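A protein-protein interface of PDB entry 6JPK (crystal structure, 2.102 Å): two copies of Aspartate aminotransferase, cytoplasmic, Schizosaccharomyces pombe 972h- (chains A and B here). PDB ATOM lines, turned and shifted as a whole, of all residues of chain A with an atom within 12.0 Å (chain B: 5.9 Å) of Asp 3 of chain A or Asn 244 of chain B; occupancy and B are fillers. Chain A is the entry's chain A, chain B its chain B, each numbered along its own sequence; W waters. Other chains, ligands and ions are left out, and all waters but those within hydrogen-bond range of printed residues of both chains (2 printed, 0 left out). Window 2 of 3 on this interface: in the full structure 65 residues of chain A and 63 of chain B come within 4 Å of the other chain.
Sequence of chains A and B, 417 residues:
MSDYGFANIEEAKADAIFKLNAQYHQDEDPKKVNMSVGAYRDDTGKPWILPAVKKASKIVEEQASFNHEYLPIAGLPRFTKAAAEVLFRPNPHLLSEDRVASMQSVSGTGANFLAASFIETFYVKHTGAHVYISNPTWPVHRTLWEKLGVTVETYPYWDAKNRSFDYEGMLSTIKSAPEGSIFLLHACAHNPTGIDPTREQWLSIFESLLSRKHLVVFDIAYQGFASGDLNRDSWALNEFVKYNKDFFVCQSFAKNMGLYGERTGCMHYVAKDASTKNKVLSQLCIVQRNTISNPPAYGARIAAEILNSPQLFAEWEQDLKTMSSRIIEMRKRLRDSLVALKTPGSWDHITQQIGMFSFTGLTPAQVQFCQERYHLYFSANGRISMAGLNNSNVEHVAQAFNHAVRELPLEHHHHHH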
ATOM      1  N   SER A   2     -14.520  11.730 -16.962  1.00  0.00           N
ATOM      2  CA  SER A   2     -15.387  12.496 -16.051  1.00  0.00           C
ATOM      3  C   SER A   2     -15.681  13.915 -16.522  1.00  0.00           C
ATOM      4  O   SER A   2     -16.804  14.396 -16.372  1.00  0.00           O
ATOM      5  CB  SER A   2     -14.795  12.587 -14.670  1.00  0.00           C
ATOM      6  OG  SER A   2     -15.738  13.208 -13.811  1.00  0.00           O
ATOM      7  N   ASP A   3     -14.672  14.606 -17.052  1.00  0.00           N
ATOM      8  CA  ASP A   3     -14.982  15.594 -18.077  1.00  0.00           C
ATOM      9  C   ASP A   3     -15.251  14.924 -19.420  1.00  0.00           C
ATOM     10  O   ASP A   3     -15.515  15.611 -20.411  1.00  0.00           O
ATOM     11  CB  ASP A   3     -13.850  16.613 -18.208  1.00  0.00           C
ATOM     12  CG  ASP A   3     -13.594  17.373 -16.916  1.00  0.00           C
ATOM     13  OD1 ASP A   3     -12.495  17.209 -16.343  1.00  0.00           O
ATOM     14  OD2 ASP A   3     -14.491  18.124 -16.469  1.00  0.00           O
ATOM     15  N   TYR A   4     -15.211  13.589 -19.455  1.00  0.00           N
ATOM     16  CA  TYR A   4     -15.251  12.798 -20.677  1.00  0.00           C
ATOM     17  C   TYR A   4     -16.265  11.661 -20.567  1.00  0.00           C
ATOM     18  O   TYR A   4     -16.213  10.701 -21.349  1.00  0.00           O
ATOM     19  CB  TYR A   4     -13.848  12.265 -21.001  1.00  0.00           C
ATOM     20  CG  TYR A   4     -12.818  13.376 -21.075  1.00  0.00           C
ATOM     21  CD1 TYR A   4     -12.689  14.151 -22.224  1.00  0.00           C
ATOM     22  CD2 TYR A   4     -11.995  13.667 -19.987  1.00  0.00           C
ATOM     23  CE1 TYR A   4     -11.765  15.187 -22.294  1.00  0.00           C
ATOM     24  CE2 TYR A   4     -11.060  14.693 -20.047  1.00  0.00           C
ATOM     25  CZ  TYR A   4     -10.953  15.452 -21.204  1.00  0.00           C
ATOM     26  OH  TYR A   4     -10.035  16.474 -21.278  1.00  0.00           O
ATOM     27  N   GLY A   5     -17.181  11.743 -19.600  1.00  0.00           N
ATOM     28  CA  GLY A   5     -18.270  10.795 -19.498  1.00  0.00           C
ATOM     29  C   GLY A   5     -17.980   9.534 -18.716  1.00  0.00           C
ATOM     30  O   GLY A   5     -18.857   8.658 -18.650  1.00  0.00           O
ATOM     31  N   PHE A   6     -16.790   9.410 -18.109  1.00  0.00           N
ATOM     32  CA  PHE A   6     -16.398   8.134 -17.515  1.00  0.00           C
ATOM     33  C   PHE A   6     -17.127   7.845 -16.209  1.00  0.00           C
ATOM     34  O   PHE A   6     -17.157   6.688 -15.784  1.00  0.00           O
ATOM     35  CB  PHE A   6     -14.884   8.081 -17.303  1.00  0.00           C
ATOM     36  CG  PHE A   6     -14.090   8.111 -18.592  1.00  0.00           C
ATOM     37  CD1 PHE A   6     -14.518   7.401 -19.705  1.00  0.00           C
ATOM     38  CD2 PHE A   6     -12.935   8.867 -18.695  1.00  0.00           C
ATOM     39  CE1 PHE A   6     -13.808   7.432 -20.889  1.00  0.00           C
ATOM     40  CE2 PHE A   6     -12.212   8.911 -19.892  1.00  0.00           C
ATOM     41  CZ  PHE A   6     -12.649   8.189 -20.986  1.00  0.00           C
ATOM     42  N   ALA A   7     -17.719   8.855 -15.571  1.00  0.00           N
ATOM     43  CA  ALA A   7     -18.538   8.607 -14.392  1.00  0.00           C
ATOM     44  C   ALA A   7     -19.847   7.904 -14.725  1.00  0.00           C
ATOM     45  O   ALA A   7     -20.490   7.381 -13.812  1.00  0.00           O
ATOM     46  CB  ALA A   7     -18.828   9.920 -13.661  1.00  0.00           C
ATOM     47  N   ASN A   8     -20.246   7.862 -16.001  1.00  0.00           N
ATOM     48  CA  ASN A   8     -21.440   7.131 -16.426  1.00  0.00           C
ATOM     49  C   ASN A   8     -21.212   5.632 -16.537  1.00  0.00           C
ATOM     50  O   ASN A   8     -22.185   4.880 -16.651  1.00  0.00           O
ATOM     51  CB  ASN A   8     -21.932   7.647 -17.781  1.00  0.00           C
ATOM     52  CG  ASN A   8     -22.263   9.124 -17.760  1.00  0.00           C
ATOM     53  OD1 ASN A   8     -22.630   9.675 -16.725  1.00  0.00           O
ATOM     54  ND2 ASN A   8     -22.135   9.774 -18.912  1.00  0.00           N
ATOM     55  N   ILE A   9     -19.955   5.185 -16.529  1.00  0.00           N
ATOM     56  CA  ILE A   9     -19.655   3.759 -16.585  1.00  0.00           C
ATOM     57  C   ILE A   9     -20.281   3.041 -15.392  1.00  0.00           C
ATOM     58  O   ILE A   9     -20.326   3.570 -14.272  1.00  0.00           O
ATOM     59  CB  ILE A   9     -18.129   3.565 -16.620  1.00  0.00           C
ATOM     60  CG1 ILE A   9     -17.552   4.130 -17.922  1.00  0.00           C
ATOM     61  CG2 ILE A   9     -17.756   2.101 -16.429  1.00  0.00           C
ATOM     62  CD1 ILE A   9     -16.037   4.083 -17.981  1.00  0.00           C
ATOM     63  N   ARG B  99      -7.222   8.653  -6.363  1.00  0.00           N
ATOM     64  CA  ARG B  99      -7.700   9.114  -7.653  1.00  0.00           C
ATOM     65  C   ARG B  99      -7.023   8.436  -8.839  1.00  0.00           C
ATOM     66  O   ARG B  99      -7.485   8.605  -9.965  1.00  0.00           O
ATOM     67  CB  ARG B  99      -7.533  10.638  -7.756  1.00  0.00           C
ATOM     68  CG  ARG B  99      -8.645  11.411  -7.010  1.00  0.00           C
ATOM     69  CD  ARG B  99      -8.339  12.884  -6.902  1.00  0.00           C
ATOM     70  NE  ARG B  99      -8.194  13.507  -8.211  1.00  0.00           N
ATOM     71  CZ  ARG B  99      -7.829  14.771  -8.390  1.00  0.00           C
ATOM     72  NH1 ARG B  99      -7.571  15.537  -7.341  1.00  0.00           N
ATOM     73  NH2 ARG B  99      -7.711  15.270  -9.614  1.00  0.00           N
ATOM     74  N   PHE B 240       0.219  19.529 -16.119  1.00  0.00           N
ATOM     75  CA  PHE B 240      -1.141  19.295 -16.590  1.00  0.00           C
ATOM     76  C   PHE B 240      -2.103  19.005 -15.444  1.00  0.00           C
ATOM     77  O   PHE B 240      -3.301  19.289 -15.565  1.00  0.00           O
ATOM     78  CB  PHE B 240      -1.169  18.152 -17.599  1.00  0.00           C
ATOM     79  CG  PHE B 240      -2.497  17.992 -18.291  1.00  0.00           C
ATOM     80  CD1 PHE B 240      -2.906  18.909 -19.247  1.00  0.00           C
ATOM     81  CD2 PHE B 240      -3.331  16.924 -17.990  1.00  0.00           C
ATOM     82  CE1 PHE B 240      -4.133  18.767 -19.888  1.00  0.00           C
ATOM     83  CE2 PHE B 240      -4.563  16.774 -18.634  1.00  0.00           C
ATOM     84  CZ  PHE B 240      -4.961  17.694 -19.578  1.00  0.00           C
ATOM     85  N   VAL B 241      -1.599  18.444 -14.337  1.00  0.00           N
ATOM     86  CA  VAL B 241      -2.419  18.183 -13.153  1.00  0.00           C
ATOM     87  C   VAL B 241      -3.086  19.460 -12.657  1.00  0.00           C
ATOM     88  O   VAL B 241      -4.205  19.420 -12.127  1.00  0.00           O
ATOM     89  CB  VAL B 241      -1.559  17.533 -12.045  1.00  0.00           C
ATOM     90  CG1 VAL B 241      -2.344  17.410 -10.732  1.00  0.00           C
ATOM     91  CG2 VAL B 241      -1.065  16.171 -12.485  1.00  0.00           C
ATOM     92  N   LYS B 242      -2.429  20.613 -12.838  1.00  0.00           N
ATOM     93  CA  LYS B 242      -3.006  21.876 -12.386  1.00  0.00           C
ATOM     94  C   LYS B 242      -4.332  22.184 -13.079  1.00  0.00           C
ATOM     95  O   LYS B 242      -5.179  22.881 -12.509  1.00  0.00           O
ATOM     96  CB  LYS B 242      -2.019  23.021 -12.622  1.00  0.00           C
ATOM     97  CG  LYS B 242      -0.665  22.815 -11.972  1.00  0.00           C
ATOM     98  CD  LYS B 242       0.276  23.965 -12.296  1.00  0.00           C
ATOM     99  CE  LYS B 242       1.589  23.819 -11.546  1.00  0.00           C
ATOM    100  NZ  LYS B 242       2.506  24.966 -11.832  1.00  0.00           N
ATOM    101  N   TYR B 243      -4.537  21.675 -14.295  1.00  0.00           N
ATOM    102  CA  TYR B 243      -5.713  22.036 -15.079  1.00  0.00           C
ATOM    103  C   TYR B 243      -6.977  21.286 -14.663  1.00  0.00           C
ATOM    104  O   TYR B 243      -8.061  21.633 -15.143  1.00  0.00           O
ATOM    105  CB  TYR B 243      -5.426  21.815 -16.567  1.00  0.00           C
ATOM    106  CG  TYR B 243      -4.348  22.737 -17.093  1.00  0.00           C
ATOM    107  CD1 TYR B 243      -3.004  22.386 -17.027  1.00  0.00           C
ATOM    108  CD2 TYR B 243      -4.671  23.973 -17.630  1.00  0.00           C
ATOM    109  CE1 TYR B 243      -2.010  23.243 -17.490  1.00  0.00           C
ATOM    110  CE2 TYR B 243      -3.681  24.832 -18.106  1.00  0.00           C
ATOM    111  CZ  TYR B 243      -2.359  24.462 -18.027  1.00  0.00           C
ATOM    112  OH  TYR B 243      -1.388  25.319 -18.494  1.00  0.00           O
ATOM    113  N   ASN B 244      -6.868  20.280 -13.794  1.00  0.00           N
ATOM    114  CA  ASN B 244      -8.023  19.595 -13.209  1.00  0.00           C
ATOM    115  C   ASN B 244      -8.922  18.958 -14.270  1.00  0.00           C
ATOM    116  O   ASN B 244     -10.147  19.133 -14.268  1.00  0.00           O
ATOM    117  CB  ASN B 244      -8.826  20.544 -12.321  1.00  0.00           C
ATOM    118  CG  ASN B 244      -8.031  21.031 -11.144  1.00  0.00           C
ATOM    119  OD1 ASN B 244      -7.679  20.249 -10.260  1.00  0.00           O
ATOM    120  ND2 ASN B 244      -7.740  22.328 -11.117  1.00  0.00           N
ATOM    121  N   LYS B 245      -8.303  18.207 -15.178  1.00  0.00           N
ATOM    122  CA  LYS B 245      -9.003  17.345 -16.121  1.00  0.00           C
ATOM    123  C   LYS B 245      -8.484  15.924 -15.959  1.00  0.00           C
ATOM    124  O   LYS B 245      -7.271  15.715 -15.824  1.00  0.00           O
ATOM    125  CB  LYS B 245      -8.800  17.824 -17.567  1.00  0.00           C
ATOM    126  CG  LYS B 245      -9.256  19.268 -17.812  1.00  0.00           C
ATOM    127  CD  LYS B 245     -10.664  19.324 -18.416  1.00  0.00           C
ATOM    128  CE  LYS B 245     -10.605  19.131 -19.936  1.00  0.00           C
ATOM    129  NZ  LYS B 245     -11.919  18.964 -20.641  1.00  0.00           N
ATOM    130  N   ASP B 246      -9.387  14.943 -15.946  1.00  0.00           N
ATOM    131  CA  ASP B 246      -8.908  13.570 -15.886  1.00  0.00           C
ATOM    132  C   ASP B 246      -8.199  13.214 -17.196  1.00  0.00           C
ATOM    133  O   ASP B 246      -8.470  13.785 -18.259  1.00  0.00           O
ATOM    134  CB  ASP B 246     -10.040  12.580 -15.541  1.00  0.00           C
ATOM    135  CG  ASP B 246     -11.357  12.830 -16.301  1.00  0.00           C
ATOM    136  OD1 ASP B 246     -11.981  11.830 -16.745  1.00  0.00           O
ATOM    137  OD2 ASP B 246     -11.789  13.994 -16.424  1.00  0.00           O
ATOM    138  N   LYS B 272     -10.842  12.230 -11.465  1.00  0.00           N
ATOM    139  CA  LYS B 272     -11.258  13.354 -10.643  1.00  0.00           C
ATOM    140  C   LYS B 272     -11.660  12.929  -9.236  1.00  0.00           C
ATOM    141  O   LYS B 272     -11.612  13.758  -8.319  1.00  0.00           O
ATOM    142  CB  LYS B 272     -12.440  14.088 -11.298  1.00  0.00           C
ATOM    143  CG  LYS B 272     -12.077  14.869 -12.554  1.00  0.00           C
ATOM    144  CD  LYS B 272     -13.280  15.623 -13.109  1.00  0.00           C
ATOM    145  CE  LYS B 272     -12.937  17.073 -13.399  1.00  0.00           C
ATOM    146  NZ  LYS B 272     -12.562  17.815 -12.177  1.00  0.00           N
HETATM  147  O   HOH W   1      -7.642  14.943 -20.595  1.00  0.00           O
HETATM  148  O   HOH W   2     -14.216  18.034 -21.715  1.00  0.00           O
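Of the 8 printed residues of chain A, 4 touch a printed residue of chain B.
Printed residues of chain A that touch a printed residue of chain B: Ser 2, Asp 3, Tyr 4 and Phe 6.
Hydrophobic or aromatic side chains of chain A within 4 Å of the printed part of chain B: Tyr 4 and Phe 6.
Of the 9 printed residues of chain B, 4 touch a printed residue of chain A.
Among the printed residues, 9 pairs touch across the chains.
Lys 272 of chain B touches Ser 2 of chain A (CD to OG, 3.5 Å).
Asp 3 of chain A touches Asn 244 of chain B.
Asp 3 of chain A touches Lys 245 of chain B.
Asp 3 of chain A touches Lys 272 of chain B (OD1 to CE, 3.0 Å).
CE2 of Tyr 4 of chain A touches O of Asp 246 of chain B, 3.3 Å away.
Phe 6 of chain A touches Asp 246 of chain B.
Of the printed residues of chain B, Ser 2 of chain A touches Asp 246 (2.6 Å) and Lys 272 (3.5 Å).
Of chain B, only Asn 244 (3.7 Å), Lys 245 (3.5 Å), Asp 246 (3.0 Å) and Lys 272 (3.0 Å) come within 4 Å of Asp 3 of chain A.
Arg 99 of chain B touches none of the printed residues of chain A.
No residue of chain A comes within 4 Å of Phe 240 of chain B.
Asn 244 of chain B touches just one residue of chain A: Asp 3 (3.7 Å).
Of the printed residues of chain A, Lys 272 of chain B touches Ser 2 (3.5 Å) and Asp 3 (3.0 Å).
The nearest residue of chain A that does not touch Asn 244 of chain B is Tyr 4 of chain A (7.3 Å).
The nearest printed residue of chain B that does not touch Ser 2 of chain A is Lys 245 of chain B (7.3 Å).
Water W2 bridges NZ of Lys 245 of chain B and O of Asp 3 of chain A.
Water W1 bridges O of Asp 246 of chain B and OH of Tyr 4 of chain A.
No position is printed for both chains.
Of the 9 pairs that touch across the chains among the printed residues, none has its exchanged pair printed and touching as well.
NE of Arg 99 of chain B lies within hydrogen-bond range of O of Lys 272 of chain B, at 3.4 Å.
The side-chain amide nitrogen (ND2) of Asn 244 of chain B lies within hydrogen-bond range of the backbone carbonyl oxygen (O) of Lys 242 of chain B (3.0 Å).
NZ of Lys 272 of chain B sits at hydrogen-bond distance from O of Asn 244 of chain B (3.5 Å).
N of Ser 2 of chain A sits at hydrogen-bond distance from OD1 of Asp 246 of chain B (2.6 Å).
N of Asp 3 of chain A is in hydrogen-bond range of OD2 of Asp 246 of chain B, 3.0 Å away.
OH of Tyr 4 of chain A sits close to NZ of Lys 245 of chain B, 3.2 Å away.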
